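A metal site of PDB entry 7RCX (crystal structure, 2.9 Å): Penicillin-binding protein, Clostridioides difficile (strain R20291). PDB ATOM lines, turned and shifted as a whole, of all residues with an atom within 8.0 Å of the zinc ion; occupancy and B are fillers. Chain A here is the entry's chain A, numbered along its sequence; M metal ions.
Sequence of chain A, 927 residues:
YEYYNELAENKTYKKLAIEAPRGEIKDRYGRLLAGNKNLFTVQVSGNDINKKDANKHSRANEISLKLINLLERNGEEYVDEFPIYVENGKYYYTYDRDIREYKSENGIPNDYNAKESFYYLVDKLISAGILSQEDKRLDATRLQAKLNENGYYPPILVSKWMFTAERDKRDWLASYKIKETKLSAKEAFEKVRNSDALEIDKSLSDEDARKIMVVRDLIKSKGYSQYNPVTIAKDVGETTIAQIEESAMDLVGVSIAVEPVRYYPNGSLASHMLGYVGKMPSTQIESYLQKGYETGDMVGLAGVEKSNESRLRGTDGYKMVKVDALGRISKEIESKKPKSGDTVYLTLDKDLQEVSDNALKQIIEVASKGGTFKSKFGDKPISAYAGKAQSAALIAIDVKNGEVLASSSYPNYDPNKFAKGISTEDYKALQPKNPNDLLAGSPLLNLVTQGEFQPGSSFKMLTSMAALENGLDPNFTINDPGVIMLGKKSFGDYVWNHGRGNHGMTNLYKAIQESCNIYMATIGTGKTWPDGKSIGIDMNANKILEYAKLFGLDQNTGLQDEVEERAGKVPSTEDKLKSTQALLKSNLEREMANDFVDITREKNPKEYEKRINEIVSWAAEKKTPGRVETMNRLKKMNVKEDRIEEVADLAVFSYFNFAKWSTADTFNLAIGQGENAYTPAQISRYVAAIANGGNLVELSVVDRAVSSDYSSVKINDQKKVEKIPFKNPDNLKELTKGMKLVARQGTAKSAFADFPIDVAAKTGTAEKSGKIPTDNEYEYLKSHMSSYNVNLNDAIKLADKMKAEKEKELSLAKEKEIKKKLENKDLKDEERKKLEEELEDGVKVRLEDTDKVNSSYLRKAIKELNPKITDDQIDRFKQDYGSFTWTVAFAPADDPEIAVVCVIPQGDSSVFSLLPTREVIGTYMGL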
ATOM      1  N   ILE A 478      -3.243  -1.536 -23.168  1.00  0.00           N
ATOM      2  CA  ILE A 478      -3.084  -0.110 -23.594  1.00  0.00           C
ATOM      3  C   ILE A 478      -3.948   0.754 -22.676  1.00  0.00           C
ATOM      4  O   ILE A 478      -5.070   0.318 -22.353  1.00  0.00           O
ATOM      5  CB  ILE A 478      -3.479   0.060 -25.078  1.00  0.00           C
ATOM      6  CG1 ILE A 478      -4.980  -0.127 -25.308  1.00  0.00           C
ATOM      7  CG2 ILE A 478      -2.659  -0.872 -25.950  1.00  0.00           C
ATOM      8  CD1 ILE A 478      -5.433   0.103 -26.727  1.00  0.00           C
ATOM      9  N   ASN A 479      -3.481   1.932 -22.281  1.00  0.00           N
ATOM     10  CA  ASN A 479      -4.367   2.961 -21.668  1.00  0.00           C
ATOM     11  C   ASN A 479      -5.119   3.656 -22.806  1.00  0.00           C
ATOM     12  O   ASN A 479      -4.530   4.556 -23.427  1.00  0.00           O
ATOM     13  CB  ASN A 479      -3.591   3.928 -20.769  1.00  0.00           C
ATOM     14  CG  ASN A 479      -4.469   5.042 -20.253  1.00  0.00           C
ATOM     15  OD1 ASN A 479      -5.704   4.933 -20.244  1.00  0.00           O
ATOM     16  ND2 ASN A 479      -3.848   6.137 -19.836  1.00  0.00           N
ATOM     17  N   ASP A 480      -6.364   3.225 -23.086  1.00  0.00           N
ATOM     18  CA  ASP A 480      -7.067   3.516 -24.374  1.00  0.00           C
ATOM     19  C   ASP A 480      -7.585   4.954 -24.348  1.00  0.00           C
ATOM     20  O   ASP A 480      -8.457   5.269 -23.543  1.00  0.00           O
ATOM     21  CB  ASP A 480      -8.197   2.534 -24.681  1.00  0.00           C
ATOM     22  CG  ASP A 480      -8.984   2.863 -25.954  1.00  0.00           C
ATOM     23  OD1 ASP A 480      -8.407   3.501 -26.855  1.00  0.00           O
ATOM     24  OD2 ASP A 480     -10.166   2.504 -26.030  1.00  0.00           O
ATOM     25  N   PRO A 481      -7.095   5.849 -25.217  1.00  0.00           N
ATOM     26  CA  PRO A 481      -7.703   7.173 -25.384  1.00  0.00           C
ATOM     27  C   PRO A 481      -8.966   7.200 -26.258  1.00  0.00           C
ATOM     28  O   PRO A 481      -9.622   8.237 -26.324  1.00  0.00           O
ATOM     29  CB  PRO A 481      -6.619   7.980 -26.110  1.00  0.00           C
ATOM     30  CG  PRO A 481      -5.852   6.937 -26.913  1.00  0.00           C
ATOM     31  CD  PRO A 481      -5.912   5.675 -26.073  1.00  0.00           C
ATOM     32  N   GLY A 482      -9.226   6.087 -26.955  1.00  0.00           N
ATOM     33  CA  GLY A 482     -10.401   5.904 -27.840  1.00  0.00           C
ATOM     34  C   GLY A 482     -10.222   6.592 -29.185  1.00  0.00           C
ATOM     35  O   GLY A 482     -11.088   6.407 -30.041  1.00  0.00           O
ATOM     36  N   VAL A 483      -9.120   7.333 -29.377  1.00  0.00           N
ATOM     37  CA  VAL A 483      -8.846   8.118 -30.618  1.00  0.00           C
ATOM     38  C   VAL A 483      -7.340   8.106 -30.905  1.00  0.00           C
ATOM     39  O   VAL A 483      -6.538   8.124 -29.944  1.00  0.00           O
ATOM     40  CB  VAL A 483      -9.363   9.555 -30.513  1.00  0.00           C
ATOM     41  CG1 VAL A 483      -8.726  10.324 -29.369  1.00  0.00           C
ATOM     42  CG2 VAL A 483      -9.209  10.328 -31.815  1.00  0.00           C
ATOM     43  N   GLY A 492     -10.969   6.846 -34.448  1.00  0.00           N
ATOM     44  CA  GLY A 492     -11.380   6.545 -33.064  1.00  0.00           C
ATOM     45  C   GLY A 492     -12.443   5.455 -32.970  1.00  0.00           C
ATOM     46  O   GLY A 492     -13.053   5.084 -33.997  1.00  0.00           O
ATOM     47  N   ASP A 493     -12.668   4.986 -31.747  1.00  0.00           N
ATOM     48  CA  ASP A 493     -13.689   3.970 -31.388  1.00  0.00           C
ATOM     49  C   ASP A 493     -15.071   4.520 -31.750  1.00  0.00           C
ATOM     50  O   ASP A 493     -15.199   5.753 -31.905  1.00  0.00           O
ATOM     51  CB  ASP A 493     -13.646   3.664 -29.884  1.00  0.00           C
ATOM     52  CG  ASP A 493     -12.371   2.968 -29.423  1.00  0.00           C
ATOM     53  OD1 ASP A 493     -11.770   2.251 -30.247  1.00  0.00           O
ATOM     54  OD2 ASP A 493     -12.015   3.123 -28.234  1.00  0.00           O
ATOM     55  N   TYR A 494     -16.055   3.643 -31.872  1.00  0.00           N
ATOM     56  CA  TYR A 494     -17.475   4.052 -32.027  1.00  0.00           C
ATOM     57  C   TYR A 494     -17.882   4.852 -30.789  1.00  0.00           C
ATOM     58  O   TYR A 494     -18.524   5.928 -30.916  1.00  0.00           O
ATOM     59  CB  TYR A 494     -18.348   2.825 -32.240  1.00  0.00           C
ATOM     60  CG  TYR A 494     -19.819   3.108 -32.299  1.00  0.00           C
ATOM     61  CD1 TYR A 494     -20.570   3.222 -31.142  1.00  0.00           C
ATOM     62  CD2 TYR A 494     -20.468   3.258 -33.513  1.00  0.00           C
ATOM     63  CE1 TYR A 494     -21.931   3.473 -31.182  1.00  0.00           C
ATOM     64  CE2 TYR A 494     -21.833   3.514 -33.581  1.00  0.00           C
ATOM     65  CZ  TYR A 494     -22.560   3.624 -32.405  1.00  0.00           C
ATOM     66  OH  TYR A 494     -23.906   3.874 -32.433  1.00  0.00           O
ATOM     67  N   VAL A 495     -17.486   4.372 -29.609  1.00  0.00           N
ATOM     68  CA  VAL A 495     -17.777   5.043 -28.309  1.00  0.00           C
ATOM     69  C   VAL A 495     -17.022   6.381 -28.239  1.00  0.00           C
ATOM     70  O   VAL A 495     -17.406   7.184 -27.370  1.00  0.00           O
ATOM     71  CB  VAL A 495     -17.440   4.164 -27.092  1.00  0.00           C
ATOM     72  CG1 VAL A 495     -18.354   2.957 -27.024  1.00  0.00           C
ATOM     73  CG2 VAL A 495     -15.975   3.760 -27.042  1.00  0.00           C
ATOM     74  N   TRP A 496     -16.000   6.605 -29.063  1.00  0.00           N
ATOM     75  CA  TRP A 496     -15.275   7.903 -29.140  1.00  0.00           C
ATOM     76  C   TRP A 496     -15.945   8.860 -30.135  1.00  0.00           C
ATOM     77  O   TRP A 496     -15.973  10.060 -29.839  1.00  0.00           O
ATOM     78  CB  TRP A 496     -13.788   7.712 -29.443  1.00  0.00           C
ATOM     79  CG  TRP A 496     -13.011   8.972 -29.185  1.00  0.00           C
ATOM     80  CD1 TRP A 496     -12.429   9.374 -28.022  1.00  0.00           C
ATOM     81  CD2 TRP A 496     -12.789  10.038 -30.130  1.00  0.00           C
ATOM     82  NE1 TRP A 496     -11.839  10.602 -28.180  1.00  0.00           N
ATOM     83  CE2 TRP A 496     -12.046  11.027 -29.462  1.00  0.00           C
ATOM     84  CE3 TRP A 496     -13.125  10.228 -31.473  1.00  0.00           C
ATOM     85  CZ2 TRP A 496     -11.635  12.200 -30.096  1.00  0.00           C
ATOM     86  CZ3 TRP A 496     -12.735  11.390 -32.099  1.00  0.00           C
ATOM     87  CH2 TRP A 496     -11.998  12.359 -31.426  1.00  0.00           C
ATOM     88  N   GLY A 501     -15.794   8.592 -25.641  1.00  0.00           N
ATOM     89  CA  GLY A 501     -15.562   7.540 -24.638  1.00  0.00           C
ATOM     90  C   GLY A 501     -14.254   6.810 -24.854  1.00  0.00           C
ATOM     91  O   GLY A 501     -13.596   7.031 -25.881  1.00  0.00           O
ATOM     92  N   ASN A 502     -13.881   5.987 -23.885  1.00  0.00           N
ATOM     93  CA  ASN A 502     -12.636   5.178 -23.904  1.00  0.00           C
ATOM     94  C   ASN A 502     -13.000   3.761 -23.475  1.00  0.00           C
ATOM     95  O   ASN A 502     -14.142   3.520 -23.036  1.00  0.00           O
ATOM     96  CB  ASN A 502     -11.556   5.737 -22.976  1.00  0.00           C
ATOM     97  CG  ASN A 502     -11.428   7.248 -23.077  1.00  0.00           C
ATOM     98  OD1 ASN A 502     -11.319   7.819 -24.172  1.00  0.00           O
ATOM     99  ND2 ASN A 502     -11.444   7.932 -21.928  1.00  0.00           N
ATOM    100  N   HIS A 503     -12.043   2.856 -23.612  1.00  0.00           N
ATOM    101  CA  HIS A 503     -12.146   1.464 -23.137  1.00  0.00           C
ATOM    102  C   HIS A 503     -11.235   1.307 -21.933  1.00  0.00           C
ATOM    103  O   HIS A 503     -10.935   0.154 -21.563  1.00  0.00           O
ATOM    104  CB  HIS A 503     -11.838   0.487 -24.274  1.00  0.00           C
ATOM    105  CG  HIS A 503     -12.849   0.596 -25.359  1.00  0.00           C
ATOM    106  ND1 HIS A 503     -12.523   0.906 -26.667  1.00  0.00           N
ATOM    107  CD2 HIS A 503     -14.193   0.511 -25.306  1.00  0.00           C
ATOM    108  CE1 HIS A 503     -13.633   0.971 -27.373  1.00  0.00           C
ATOM    109  NE2 HIS A 503     -14.671   0.729 -26.565  1.00  0.00           N
ATOM    110  N   GLY A 504     -10.804   2.428 -21.355  1.00  0.00           N
ATOM    111  CA  GLY A 504      -9.901   2.429 -20.199  1.00  0.00           C
ATOM    112  C   GLY A 504      -8.723   1.505 -20.470  1.00  0.00           C
ATOM    113  O   GLY A 504      -8.141   1.613 -21.563  1.00  0.00           O
ATOM    114  N   THR A 506      -7.130  -1.885 -21.572  1.00  0.00           N
ATOM    115  CA  THR A 506      -7.635  -2.891 -22.542  1.00  0.00           C
ATOM    116  C   THR A 506      -6.541  -3.878 -22.943  1.00  0.00           C
ATOM    117  O   THR A 506      -5.547  -3.427 -23.522  1.00  0.00           O
ATOM    118  CB  THR A 506      -8.130  -2.197 -23.810  1.00  0.00           C
ATOM    119  OG1 THR A 506      -8.964  -1.087 -23.479  1.00  0.00           O
ATOM    120  CG2 THR A 506      -8.916  -3.121 -24.723  1.00  0.00           C
ATOM    121  N   LYS A 510     -10.590  -7.631 -24.048  1.00  0.00           N
ATOM    122  CA  LYS A 510     -11.455  -6.412 -23.985  1.00  0.00           C
ATOM    123  C   LYS A 510     -11.565  -5.749 -25.373  1.00  0.00           C
ATOM    124  O   LYS A 510     -12.682  -5.328 -25.747  1.00  0.00           O
ATOM    125  CB  LYS A 510     -10.931  -5.441 -22.914  1.00  0.00           C
ATOM    126  CG  LYS A 510     -11.889  -4.345 -22.492  1.00  0.00           C
ATOM    127  CD  LYS A 510     -11.430  -3.577 -21.270  1.00  0.00           C
ATOM    128  CE  LYS A 510     -12.574  -2.831 -20.596  1.00  0.00           C
ATOM    129  NZ  LYS A 510     -12.088  -1.886 -19.560  1.00  0.00           N
ATOM    130  N   ALA A 511     -10.460  -5.638 -26.107  1.00  0.00           N
ATOM    131  CA  ALA A 511     -10.397  -5.134 -27.509  1.00  0.00           C
ATOM    132  C   ALA A 511     -11.471  -5.828 -28.349  1.00  0.00           C
ATOM    133  O   ALA A 511     -12.260  -5.115 -28.985  1.00  0.00           O
ATOM    134  CB  ALA A 511      -9.041  -5.365 -28.104  1.00  0.00           C
ATOM    135  N   GLU A 514     -15.246  -5.349 -26.747  1.00  0.00           N
ATOM    136  CA  GLU A 514     -15.808  -3.981 -26.870  1.00  0.00           C
ATOM    137  C   GLU A 514     -15.576  -3.434 -28.284  1.00  0.00           C
ATOM    138  O   GLU A 514     -16.088  -2.353 -28.590  1.00  0.00           O
ATOM    139  CB  GLU A 514     -15.158  -3.065 -25.835  1.00  0.00           C
ATOM    140  CG  GLU A 514     -15.521  -3.383 -24.402  1.00  0.00           C
ATOM    141  CD  GLU A 514     -16.997  -3.224 -24.084  1.00  0.00           C
ATOM    142  OE1 GLU A 514     -17.633  -2.359 -24.715  1.00  0.00           O
ATOM    143  OE2 GLU A 514     -17.514  -3.976 -23.227  1.00  0.00           O
ATOM    144  N   SER A 515     -14.837  -4.157 -29.139  1.00  0.00           N
ATOM    145  CA  SER A 515     -14.440  -3.660 -30.479  1.00  0.00           C
ATOM    146  C   SER A 515     -13.653  -2.345 -30.323  1.00  0.00           C
ATOM    147  O   SER A 515     -14.193  -1.264 -30.625  1.00  0.00           O
ATOM    148  CB  SER A 515     -15.644  -3.517 -31.379  1.00  0.00           C
ATOM    149  OG  SER A 515     -15.264  -3.684 -32.739  1.00  0.00           O
ATOM    150  N   CYS A 516     -12.428  -2.451 -29.815  1.00  0.00           N
ATOM    151  CA  CYS A 516     -11.464  -1.331 -29.700  1.00  0.00           C
ATOM    152  C   CYS A 516     -10.718  -1.186 -31.042  1.00  0.00           C
ATOM    153  O   CYS A 516      -9.827  -2.021 -31.312  1.00  0.00           O
ATOM    154  CB  CYS A 516     -10.500  -1.553 -28.539  1.00  0.00           C
ATOM    155  SG  CYS A 516      -9.440  -0.119 -28.210  1.00  0.00           S
ATOM    156  N   ASN A 517     -11.083  -0.175 -31.835  1.00  0.00           N
ATOM    157  CA  ASN A 517     -10.419   0.192 -33.108  1.00  0.00           C
ATOM    158  C   ASN A 517      -8.964   0.561 -32.810  1.00  0.00           C
ATOM    159  O   ASN A 517      -8.044   0.170 -33.573  1.00  0.00           O
ATOM    160  CB  ASN A 517     -11.162   1.312 -33.828  1.00  0.00           C
ATOM    161  CG  ASN A 517     -12.544   0.898 -34.305  1.00  0.00           C
ATOM    162  OD1 ASN A 517     -12.834  -0.293 -34.392  1.00  0.00           O
ATOM    163  ND2 ASN A 517     -13.420   1.853 -34.588  1.00  0.00           N
ATOM    164  N   ILE A 518      -8.763   1.271 -31.689  1.00  0.00           N
ATOM    165  CA  ILE A 518      -7.429   1.827 -31.294  1.00  0.00           C
ATOM    166  C   ILE A 518      -6.482   0.656 -31.050  1.00  0.00           C
ATOM    167  O   ILE A 518      -5.363   0.682 -31.618  1.00  0.00           O
ATOM    168  CB  ILE A 518      -7.547   2.730 -30.052  1.00  0.00           C
ATOM    169  CG1 ILE A 518      -8.614   3.812 -30.237  1.00  0.00           C
ATOM    170  CG2 ILE A 518      -6.189   3.323 -29.697  1.00  0.00           C
ATOM    171  CD1 ILE A 518      -8.555   4.508 -31.575  1.00  0.00           C
ATOM    172  N   TYR A 519      -6.900  -0.329 -30.252  1.00  0.00           N
ATOM    173  CA  TYR A 519      -6.122  -1.551 -29.946  1.00  0.00           C
ATOM    174  C   TYR A 519      -5.815  -2.293 -31.244  1.00  0.00           C
ATOM    175  O   TYR A 519      -4.679  -2.767 -31.418  1.00  0.00           O
ATOM    176  CB  TYR A 519      -6.865  -2.470 -28.987  1.00  0.00           C
ATOM    177  CG  TYR A 519      -5.994  -3.541 -28.390  1.00  0.00           C
ATOM    178  CD1 TYR A 519      -5.570  -4.623 -29.138  1.00  0.00           C
ATOM    179  CD2 TYR A 519      -5.567  -3.454 -27.074  1.00  0.00           C
ATOM    180  CE1 TYR A 519      -4.750  -5.596 -28.593  1.00  0.00           C
ATOM    181  CE2 TYR A 519      -4.739  -4.418 -26.522  1.00  0.00           C
ATOM    182  CZ  TYR A 519      -4.330  -5.489 -27.281  1.00  0.00           C
ATOM    183  OH  TYR A 519      -3.520  -6.459 -26.756  1.00  0.00           O
ATOM    184  N   MET A 520      -6.794  -2.392 -32.139  1.00  0.00           N
ATOM    185  CA  MET A 520      -6.641  -3.128 -33.418  1.00  0.00           C
ATOM    186  C   MET A 520      -5.583  -2.434 -34.272  1.00  0.00           C
ATOM    187  O   MET A 520      -4.753  -3.160 -34.822  1.00  0.00           O
ATOM    188  CB  MET A 520      -7.962  -3.227 -34.189  1.00  0.00           C
ATOM    189  CG  MET A 520      -8.887  -4.263 -33.614  1.00  0.00           C
ATOM    190  SD  MET A 520      -8.065  -5.850 -33.365  1.00  0.00           S
ATOM    191  CE  MET A 520      -8.985  -6.462 -31.947  1.00  0.00           C
HETATM  192 ZN    ZN M   1     -11.041   1.354 -27.410  1.00  0.00          ZN
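The side-chain hydroxyl (OG1) of Thr 506 sits at hydrogen-bond distance from the backbone carbonyl oxygen (O) of His 503 (3.0 Å). OD1 of Asp 480 sits at hydrogen-bond distance from N of Gly 482 (2.7 Å). N of Asp 480 lies within hydrogen-bond range of O of Gly 504 (2.8 Å). The side-chain carboxylate (OD1) of Asp 493 sits at hydrogen-bond distance from the backbone NH (N) of Ile 518, at 3.5 Å. The backbone carbonyl oxygen (O) of Gly 482 is in hydrogen-bond range of the backbone NH (N) of Asp 493, at 2.7 Å. The backbone NH of Asn 517 sits at hydrogen-bond distance from the side-chain carboxylate of Asp 493 (3.0 Å). SG of Cys 516 sits close to N of Tyr 519 (3.3 Å). The backbone carbonyl oxygen (O) of Ala 511 sits at hydrogen-bond distance from the backbone NH (N) of Cys 516, 2.8 Å away.
The nearest printed residue that does not touch the zinc ion is Ile 518 (4.5 Å).
ND1 of His 503 binds the zinc ion. The zinc ion is bound by OD2 of Asp 480. OD2 of Asp 493 is bound to the zinc ion, 2.2 Å away. The side-chain sulfur (SG) of Cys 516 binds the zinc ion, at 2.3 Å. The zinc ion has four donor atoms within binding distance.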
